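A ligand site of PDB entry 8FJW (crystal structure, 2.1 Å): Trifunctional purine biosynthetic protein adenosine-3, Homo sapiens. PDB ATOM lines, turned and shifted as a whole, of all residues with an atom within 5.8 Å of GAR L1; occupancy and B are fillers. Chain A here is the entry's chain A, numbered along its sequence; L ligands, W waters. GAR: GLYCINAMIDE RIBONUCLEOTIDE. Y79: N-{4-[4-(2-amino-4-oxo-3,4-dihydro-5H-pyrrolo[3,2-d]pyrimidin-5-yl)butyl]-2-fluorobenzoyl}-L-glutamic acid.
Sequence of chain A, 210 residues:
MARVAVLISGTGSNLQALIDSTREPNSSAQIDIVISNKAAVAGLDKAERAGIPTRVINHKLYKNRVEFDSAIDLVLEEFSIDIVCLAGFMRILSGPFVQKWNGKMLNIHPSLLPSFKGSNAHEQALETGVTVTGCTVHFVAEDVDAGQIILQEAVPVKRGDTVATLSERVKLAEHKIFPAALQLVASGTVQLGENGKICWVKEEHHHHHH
The backbone carbonyl oxygen (O) of Ile 108 lies within hydrogen-bond range of a nitrogen (N24) of GAR L1 (3.4 Å). The backbone NH (N) of Ser 13 lies within hydrogen-bond range of an oxygen (O17) of GAR L1 (2.8 Å). NZ of Lys 171 lies within salt-bridge range of O17 of GAR L1, at 3.0 Å. A ring nitrogen (ND1) of His 109 is in hydrogen-bond range of a nitrogen (N24) of GAR L1, 3.1 Å away. O16 of GAR L1 is in hydrogen-bond range of N of Asn 14. O of Met 90 sits close to N19 of Y79 L2, at 3.5 Å. N of Gly 12 sits at hydrogen-bond distance from O18 of GAR L1. The side-chain carboxylate (OE2) of Glu 174 is in hydrogen-bond range of an oxygen (O6) of GAR L1. OG of Ser 13 lies within hydrogen-bond range of O17 of GAR L1 (2.4 Å). The side-chain amide nitrogen (ND2) of Asn 14 lies within hydrogen-bond range of an oxygen (O16) of GAR L1 (3.0 Å).
OG of Ser 13 is in hydrogen-bond range of NE2 of His 175. A ring nitrogen (ND1) of His 175 sits close to the backbone carbonyl oxygen of Lys 171 (3.3 Å). The side-chain amide nitrogen (ND2) of Asn 14 sits at hydrogen-bond distance from the side-chain carboxylate (OE2) of Glu 174 (2.8 Å).
O8 of GAR L1 lies close to N of Pro 110. Thr 11 touches GAR L1. Gly 88 touches GAR L1. Met 90 touches GAR L1 (CE to O4, 3.1 Å). Asn 107 touches GAR L1.
Water W6 lies within hydrogen-bond range of an oxygen (O16) of GAR L1, the backbone carbonyl oxygen (O) of Ala 87, the backbone NH (N) of Leu 15 and the backbone NH (N) of Asn 14. Water W3 lies within hydrogen-bond range of an oxygen (O18) of GAR L1 (2.7 Å), the backbone NH of Gly 10 (2.8 Å) and the backbone carbonyl oxygen of Ala 87 (3.1 Å). Water W5 bridges O6 of GAR L1 (2.7 Å) and NE2 of His 122 (3.4 Å). Water W4 bridges O18 of GAR L1 (2.7 Å) and N of Thr 11 (3.0 Å). Water W2 lies within hydrogen-bond range of a ring nitrogen (NE2) of His 122, the side-chain carboxylate (OE1) of Glu 174, the backbone carbonyl oxygen (O) of Ser 167 and an oxygen (O6) of GAR L1.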
ATOM      1  N   GLY A  10      19.099 -31.469   1.845  1.00  0.00           N
ATOM      2  CA  GLY A  10      20.322 -31.172   1.133  1.00  0.00           C
ATOM      3  C   GLY A  10      21.561 -31.054   1.991  1.00  0.00           C
ATOM      4  O   GLY A  10      21.884 -31.975   2.755  1.00  0.00           O
ATOM      5  N   THR A  11      22.266 -29.924   1.871  1.00  0.00           N
ATOM      6  CA  THR A  11      23.605 -29.809   2.445  1.00  0.00           C
ATOM      7  C   THR A  11      23.588 -29.964   3.963  1.00  0.00           C
ATOM      8  O   THR A  11      24.469 -30.617   4.534  1.00  0.00           O
ATOM      9  CB  THR A  11      24.221 -28.474   2.052  1.00  0.00           C
ATOM     10  OG1 THR A  11      24.265 -28.363   0.624  1.00  0.00           O
ATOM     11  CG2 THR A  11      25.640 -28.352   2.604  1.00  0.00           C
ATOM     12  N   GLY A  12      22.622 -29.354   4.632  1.00  0.00           N
ATOM     13  CA  GLY A  12      22.488 -29.513   6.068  1.00  0.00           C
ATOM     14  C   GLY A  12      23.372 -28.611   6.907  1.00  0.00           C
ATOM     15  O   GLY A  12      23.699 -28.967   8.046  1.00  0.00           O
ATOM     16  N   SER A  13      23.783 -27.452   6.380  1.00  0.00           N
ATOM     17  CA  SER A  13      24.536 -26.507   7.196  1.00  0.00           C
ATOM     18  C   SER A  13      23.718 -26.053   8.395  1.00  0.00           C
ATOM     19  O   SER A  13      24.255 -25.878   9.495  1.00  0.00           O
ATOM     20  CB  SER A  13      24.990 -25.312   6.360  1.00  0.00           C
ATOM     21  OG  SER A  13      23.886 -24.566   5.875  1.00  0.00           O
ATOM     22  N   ASN A  14      22.413 -25.858   8.211  1.00  0.00           N
ATOM     23  CA  ASN A  14      21.579 -25.512   9.366  1.00  0.00           C
ATOM     24  C   ASN A  14      21.518 -26.678  10.348  1.00  0.00           C
ATOM     25  O   ASN A  14      21.570 -26.461  11.569  1.00  0.00           O
ATOM     26  CB  ASN A  14      20.185 -25.097   8.913  1.00  0.00           C
ATOM     27  CG  ASN A  14      20.117 -23.632   8.517  1.00  0.00           C
ATOM     28  OD1 ASN A  14      20.173 -22.743   9.368  1.00  0.00           O
ATOM     29  ND2 ASN A  14      19.997 -23.377   7.220  1.00  0.00           N
ATOM     30  N   LEU A  15      21.400 -27.905   9.842  1.00  0.00           N
ATOM     31  CA  LEU A  15      21.459 -29.066  10.731  1.00  0.00           C
ATOM     32  C   LEU A  15      22.714 -29.046  11.578  1.00  0.00           C
ATOM     33  O   LEU A  15      22.674 -29.261  12.788  1.00  0.00           O
ATOM     34  CB  LEU A  15      21.377 -30.357   9.914  1.00  0.00           C
ATOM     35  CG  LEU A  15      21.585 -31.648  10.713  1.00  0.00           C
ATOM     36  CD1 LEU A  15      20.518 -31.792  11.796  1.00  0.00           C
ATOM     37  CD2 LEU A  15      21.601 -32.860   9.794  1.00  0.00           C
ATOM     38  N   ALA A  87      14.905 -27.964   8.330  1.00  0.00           N
ATOM     39  CA  ALA A  87      16.199 -27.345   8.033  1.00  0.00           C
ATOM     40  C   ALA A  87      16.569 -27.674   6.592  1.00  0.00           C
ATOM     41  O   ALA A  87      17.332 -28.603   6.329  1.00  0.00           O
ATOM     42  CB  ALA A  87      17.278 -27.809   9.021  1.00  0.00           C
ATOM     43  N   GLY A  88      16.024 -26.887   5.658  1.00  0.00           N
ATOM     44  CA  GLY A  88      16.221 -27.178   4.252  1.00  0.00           C
ATOM     45  C   GLY A  88      15.329 -28.265   3.713  1.00  0.00           C
ATOM     46  O   GLY A  88      15.696 -28.905   2.717  1.00  0.00           O
ATOM     47  N   PHE A  89      14.184 -28.507   4.340  1.00  0.00           N
ATOM     48  CA  PHE A  89      13.237 -29.519   3.891  1.00  0.00           C
ATOM     49  C   PHE A  89      12.381 -28.926   2.790  1.00  0.00           C
ATOM     50  O   PHE A  89      11.549 -28.048   3.038  1.00  0.00           O
ATOM     51  CB  PHE A  89      12.395 -30.010   5.063  1.00  0.00           C
ATOM     52  CG  PHE A  89      11.581 -31.239   4.767  1.00  0.00           C
ATOM     53  CD1 PHE A  89      12.200 -32.458   4.573  1.00  0.00           C
ATOM     54  CD2 PHE A  89      10.205 -31.176   4.703  1.00  0.00           C
ATOM     55  CE1 PHE A  89      11.465 -33.597   4.307  1.00  0.00           C
ATOM     56  CE2 PHE A  89       9.452 -32.302   4.441  1.00  0.00           C
ATOM     57  CZ  PHE A  89      10.088 -33.519   4.246  1.00  0.00           C
ATOM     58  N   MET A  90      12.565 -29.406   1.551  1.00  0.00           N
ATOM     59  CA  MET A  90      11.918 -28.836   0.370  1.00  0.00           C
ATOM     60  C   MET A  90      10.726 -29.676  -0.073  1.00  0.00           C
ATOM     61  O   MET A  90      10.564 -29.975  -1.257  1.00  0.00           O
ATOM     62  CB  MET A  90      12.936 -28.707  -0.758  1.00  0.00           C
ATOM     63  CG  MET A  90      14.175 -27.921  -0.404  1.00  0.00           C
ATOM     64  SD  MET A  90      13.813 -26.217   0.089  1.00  0.00           S
ATOM     65  CE  MET A  90      15.476 -25.586   0.298  1.00  0.00           C
ATOM     66  N   ASN A 107      10.607 -23.686  11.163  1.00  0.00           N
ATOM     67  CA  ASN A 107      11.165 -23.638   9.816  1.00  0.00           C
ATOM     68  C   ASN A 107      12.038 -22.395   9.688  1.00  0.00           C
ATOM     69  O   ASN A 107      11.708 -21.338  10.224  1.00  0.00           O
ATOM     70  CB  ASN A 107      10.060 -23.636   8.755  1.00  0.00           C
ATOM     71  CG  ASN A 107      10.596 -23.478   7.346  1.00  0.00           C
ATOM     72  OD1 ASN A 107      11.249 -24.367   6.813  1.00  0.00           O
ATOM     73  ND2 ASN A 107      10.316 -22.325   6.737  1.00  0.00           N
ATOM     74  N   ILE A 108      13.154 -22.535   8.991  1.00  0.00           N
ATOM     75  CA  ILE A 108      14.047 -21.429   8.671  1.00  0.00           C
ATOM     76  C   ILE A 108      13.810 -21.021   7.229  1.00  0.00           C
ATOM     77  O   ILE A 108      13.846 -21.876   6.322  1.00  0.00           O
ATOM     78  CB  ILE A 108      15.522 -21.810   8.919  1.00  0.00           C
ATOM     79  CG1 ILE A 108      16.468 -20.653   8.569  1.00  0.00           C
ATOM     80  CG2 ILE A 108      15.895 -23.038   8.103  1.00  0.00           C
ATOM     81  CD1 ILE A 108      16.355 -19.467   9.497  1.00  0.00           C
ATOM     82  N   HIS A 109      13.555 -19.743   7.002  1.00  0.00           N
ATOM     83  CA  HIS A 109      13.298 -19.226   5.665  1.00  0.00           C
ATOM     84  C   HIS A 109      14.277 -18.097   5.354  1.00  0.00           C
ATOM     85  O   HIS A 109      14.435 -17.185   6.174  1.00  0.00           O
ATOM     86  CB  HIS A 109      11.844 -18.722   5.537  1.00  0.00           C
ATOM     87  CG  HIS A 109      11.467 -18.308   4.154  1.00  0.00           C
ATOM     88  ND1 HIS A 109      11.349 -19.200   3.113  1.00  0.00           N
ATOM     89  CD2 HIS A 109      11.173 -17.086   3.634  1.00  0.00           C
ATOM     90  CE1 HIS A 109      10.995 -18.557   2.015  1.00  0.00           C
ATOM     91  NE2 HIS A 109      10.885 -17.268   2.302  1.00  0.00           N
ATOM     92  N   PRO A 110      14.963 -18.128   4.185  1.00  0.00           N
ATOM     93  CA  PRO A 110      16.007 -17.147   3.870  1.00  0.00           C
ATOM     94  C   PRO A 110      15.478 -15.807   3.375  1.00  0.00           C
ATOM     95  O   PRO A 110      15.912 -15.282   2.345  1.00  0.00           O
ATOM     96  CB  PRO A 110      16.817 -17.872   2.778  1.00  0.00           C
ATOM     97  CG  PRO A 110      15.793 -18.679   2.064  1.00  0.00           C
ATOM     98  CD  PRO A 110      14.813 -19.138   3.112  1.00  0.00           C
ATOM     99  N   GLY A 118       8.061 -18.370  -0.443  1.00  0.00           N
ATOM    100  CA  GLY A 118       8.239 -19.332  -1.523  1.00  0.00           C
ATOM    101  C   GLY A 118       9.652 -19.874  -1.627  1.00  0.00           C
ATOM    102  O   GLY A 118      10.516 -19.659  -0.773  1.00  0.00           O
ATOM    103  N   SER A 119       9.885 -20.570  -2.739  1.00  0.00           N
ATOM    104  CA  SER A 119      11.044 -21.445  -2.873  1.00  0.00           C
ATOM    105  C   SER A 119      12.317 -20.724  -3.304  1.00  0.00           C
ATOM    106  O   SER A 119      13.406 -21.273  -3.107  1.00  0.00           O
ATOM    107  CB  SER A 119      10.731 -22.554  -3.862  1.00  0.00           C
ATOM    108  OG  SER A 119      10.358 -22.019  -5.123  1.00  0.00           O
ATOM    109  N   ALA A 121      13.603 -17.396  -2.447  1.00  0.00           N
ATOM    110  CA  ALA A 121      13.587 -16.097  -1.770  1.00  0.00           C
ATOM    111  C   ALA A 121      14.746 -15.223  -2.226  1.00  0.00           C
ATOM    112  O   ALA A 121      14.568 -14.024  -2.482  1.00  0.00           O
ATOM    113  CB  ALA A 121      13.623 -16.292  -0.264  1.00  0.00           C
ATOM    114  N   HIS A 122      15.939 -15.797  -2.351  1.00  0.00           N
ATOM    115  CA  HIS A 122      17.096 -15.000  -2.741  1.00  0.00           C
ATOM    116  C   HIS A 122      16.918 -14.405  -4.134  1.00  0.00           C
ATOM    117  O   HIS A 122      17.201 -13.216  -4.340  1.00  0.00           O
ATOM    118  CB  HIS A 122      18.373 -15.849  -2.681  1.00  0.00           C
ATOM    119  CG  HIS A 122      18.768 -16.230  -1.281  1.00  0.00           C
ATOM    120  ND1 HIS A 122      18.827 -15.323  -0.249  1.00  0.00           N
ATOM    121  CD2 HIS A 122      19.125 -17.423  -0.753  1.00  0.00           C
ATOM    122  CE1 HIS A 122      19.209 -15.939   0.860  1.00  0.00           C
ATOM    123  NE2 HIS A 122      19.395 -17.218   0.572  1.00  0.00           N
ATOM    124  N   SER A 167      23.089 -15.944  -0.513  1.00  0.00           N
ATOM    125  CA  SER A 167      22.713 -17.091   0.308  1.00  0.00           C
ATOM    126  C   SER A 167      23.828 -17.459   1.290  1.00  0.00           C
ATOM    127  O   SER A 167      23.554 -17.888   2.410  1.00  0.00           O
ATOM    128  CB  SER A 167      22.372 -18.285  -0.572  1.00  0.00           C
ATOM    129  OG  SER A 167      23.522 -18.757  -1.257  1.00  0.00           O
ATOM    130  N   LYS A 171      23.129 -17.439   5.272  1.00  0.00           N
ATOM    131  CA  LYS A 171      23.256 -18.674   6.034  1.00  0.00           C
ATOM    132  C   LYS A 171      24.006 -18.458   7.339  1.00  0.00           C
ATOM    133  O   LYS A 171      23.720 -19.124   8.335  1.00  0.00           O
ATOM    134  CB  LYS A 171      23.923 -19.766   5.196  1.00  0.00           C
ATOM    135  CG  LYS A 171      22.950 -20.499   4.279  1.00  0.00           C
ATOM    136  CD  LYS A 171      23.599 -21.730   3.650  1.00  0.00           C
ATOM    137  CE  LYS A 171      22.647 -22.408   2.675  1.00  0.00           C
ATOM    138  NZ  LYS A 171      23.147 -23.760   2.288  1.00  0.00           N
ATOM    139  N   GLU A 174      21.292 -17.457   9.514  1.00  0.00           N
ATOM    140  CA  GLU A 174      20.463 -18.628   9.800  1.00  0.00           C
ATOM    141  C   GLU A 174      21.076 -19.485  10.892  1.00  0.00           C
ATOM    142  O   GLU A 174      20.375 -19.933  11.813  1.00  0.00           O
ATOM    143  CB  GLU A 174      20.260 -19.450   8.521  1.00  0.00           C
ATOM    144  CG  GLU A 174      19.447 -18.760   7.442  1.00  0.00           C
ATOM    145  CD  GLU A 174      19.382 -19.571   6.165  1.00  0.00           C
ATOM    146  OE1 GLU A 174      19.246 -18.968   5.083  1.00  0.00           O
ATOM    147  OE2 GLU A 174      19.479 -20.813   6.245  1.00  0.00           O
ATOM    148  N   HIS A 175      22.385 -19.727  10.821  1.00  0.00           N
ATOM    149  CA  HIS A 175      23.068 -20.560  11.793  1.00  0.00           C
ATOM    150  C   HIS A 175      23.065 -19.959  13.188  1.00  0.00           C
ATOM    151  O   HIS A 175      23.439 -20.655  14.146  1.00  0.00           O
ATOM    152  CB  HIS A 175      24.505 -20.822  11.346  1.00  0.00           C
ATOM    153  CG  HIS A 175      24.609 -21.495  10.008  1.00  0.00           C
ATOM    154  ND1 HIS A 175      25.768 -21.504   9.268  1.00  0.00           N
ATOM    155  CD2 HIS A 175      23.690 -22.175   9.287  1.00  0.00           C
ATOM    156  CE1 HIS A 175      25.563 -22.160   8.139  1.00  0.00           C
ATOM    157  NE2 HIS A 175      24.317 -22.577   8.127  1.00  0.00           N
HETATM  158  C1  GAR L   1      18.540 -22.712   3.850  1.00  0.00           C
HETATM  159  O6  GAR L   1      19.290 -21.583   3.425  1.00  0.00           O
HETATM  160  C2  GAR L   1      17.050 -22.401   4.028  1.00  0.00           C
HETATM  161  O8  GAR L   1      16.766 -21.060   4.352  1.00  0.00           O
HETATM  162  C3  GAR L   1      16.462 -22.819   2.672  1.00  0.00           C
HETATM  163  O4  GAR L   1      17.283 -23.928   2.229  1.00  0.00           O
HETATM  164  C5  GAR L   1      18.612 -23.792   2.766  1.00  0.00           C
HETATM  165  C10 GAR L   1      19.130 -25.121   3.281  1.00  0.00           C
HETATM  166  O12 GAR L   1      20.465 -24.959   3.755  1.00  0.00           O
HETATM  167  N19 GAR L   1      15.068 -23.180   2.724  1.00  0.00           N
HETATM  168  C21 GAR L   1      14.168 -22.545   1.972  1.00  0.00           C
HETATM  169  O22 GAR L   1      14.451 -21.718   1.114  1.00  0.00           O
HETATM  170  C23 GAR L   1      12.721 -22.897   2.244  1.00  0.00           C
HETATM  171  N24 GAR L   1      12.209 -22.192   3.415  1.00  0.00           N
HETATM  172  P15 GAR L   1      21.201 -26.171   4.530  1.00  0.00           P
HETATM  173  O16 GAR L   1      20.743 -25.977   5.950  1.00  0.00           O
HETATM  174  O17 GAR L   1      22.668 -25.926   4.296  1.00  0.00           O
HETATM  175  O18 GAR L   1      20.651 -27.430   3.889  1.00  0.00           O
HETATM  176  C8  Y79 L   2       6.339 -25.790   4.850  1.00  0.00           C
HETATM  177  C5  Y79 L   2       6.951 -27.859   4.232  1.00  0.00           C
HETATM  178  C6  Y79 L   2       8.068 -27.039   4.378  1.00  0.00           C
HETATM  179  N1  Y79 L   2       4.487 -27.216   4.593  1.00  0.00           N
HETATM  180  C2  Y79 L   2       3.674 -26.216   4.923  1.00  0.00           C
HETATM  181  C4  Y79 L   2       5.439 -24.747   5.208  1.00  0.00           C
HETATM  182  C9  Y79 L   2       5.832 -27.030   4.546  1.00  0.00           C
HETATM  183  C12 Y79 L   2       8.553 -25.547  -1.816  1.00  0.00           C
HETATM  184  C13 Y79 L   2       8.054 -24.252  -1.747  1.00  0.00           C
HETATM  185  C14 Y79 L   2       9.345 -26.046  -0.805  1.00  0.00           C
HETATM  186  C15 Y79 L   2       8.353 -23.449  -0.663  1.00  0.00           C
HETATM  187  C16 Y79 L   2       9.651 -25.250   0.282  1.00  0.00           C
HETATM  188  C17 Y79 L   2       8.227 -26.456  -2.996  1.00  0.00           C
HETATM  189  C20 Y79 L   2       7.900 -28.805  -3.853  1.00  0.00           C
HETATM  190  C21 Y79 L   2       9.137 -29.653  -4.160  1.00  0.00           C
HETATM  191  C22 Y79 L   2      10.401 -28.785  -4.176  1.00  0.00           C
HETATM  192  C23 Y79 L   2      11.586 -29.472  -4.824  1.00  0.00           C
HETATM  193  C26 Y79 L   2       6.758 -29.706  -3.403  1.00  0.00           C
HETATM  194  C29 Y79 L   2       8.557 -24.693   4.999  1.00  0.00           C
HETATM  195  C30 Y79 L   2       8.512 -23.717   3.822  1.00  0.00           C
HETATM  196  C31 Y79 L   2       9.581 -24.042   2.787  1.00  0.00           C
HETATM  197  C32 Y79 L   2       9.512 -23.110   1.574  1.00  0.00           C
HETATM  198  C33 Y79 L   2       9.152 -23.955   0.350  1.00  0.00           C
HETATM  199  F34 Y79 L   2       7.256 -23.769  -2.752  1.00  0.00           F
HETATM  200  N11 Y79 L   2       2.245 -26.461   4.967  1.00  0.00           N
HETATM  201  N19 Y79 L   2       8.205 -27.892  -2.778  1.00  0.00           N
HETATM  202  N3  Y79 L   2       4.143 -25.007   5.233  1.00  0.00           N
HETATM  203  N7  Y79 L   2       7.690 -25.831   4.749  1.00  0.00           N
HETATM  204  O10 Y79 L   2       5.924 -23.482   5.527  1.00  0.00           O
HETATM  205  O18 Y79 L   2       8.000 -26.008  -4.070  1.00  0.00           O
HETATM  206  O24 Y79 L   2      11.395 -30.266  -5.783  1.00  0.00           O
HETATM  207  O25 Y79 L   2      12.751 -29.245  -4.415  1.00  0.00           O
HETATM  208  O27 Y79 L   2       5.716 -29.811  -4.105  1.00  0.00           O
HETATM  209  O28 Y79 L   2       6.844 -30.340  -2.321  1.00  0.00           O
HETATM  210  O   HOH W   1      13.382 -19.770  -0.515  1.00  0.00           O
HETATM  211  O   HOH W   2      20.659 -18.478   2.716  1.00  0.00           O
HETATM  212  O   HOH W   3      18.985 -29.504   3.861  1.00  0.00           O
HETATM  213  O   HOH W   4      20.495 -27.567   1.193  1.00  0.00           O
HETATM  214  O   HOH W   5      19.647 -20.623   0.948  1.00  0.00           O
HETATM  215  O   HOH W   6      20.018 -28.038   7.266  1.00  0.00           O
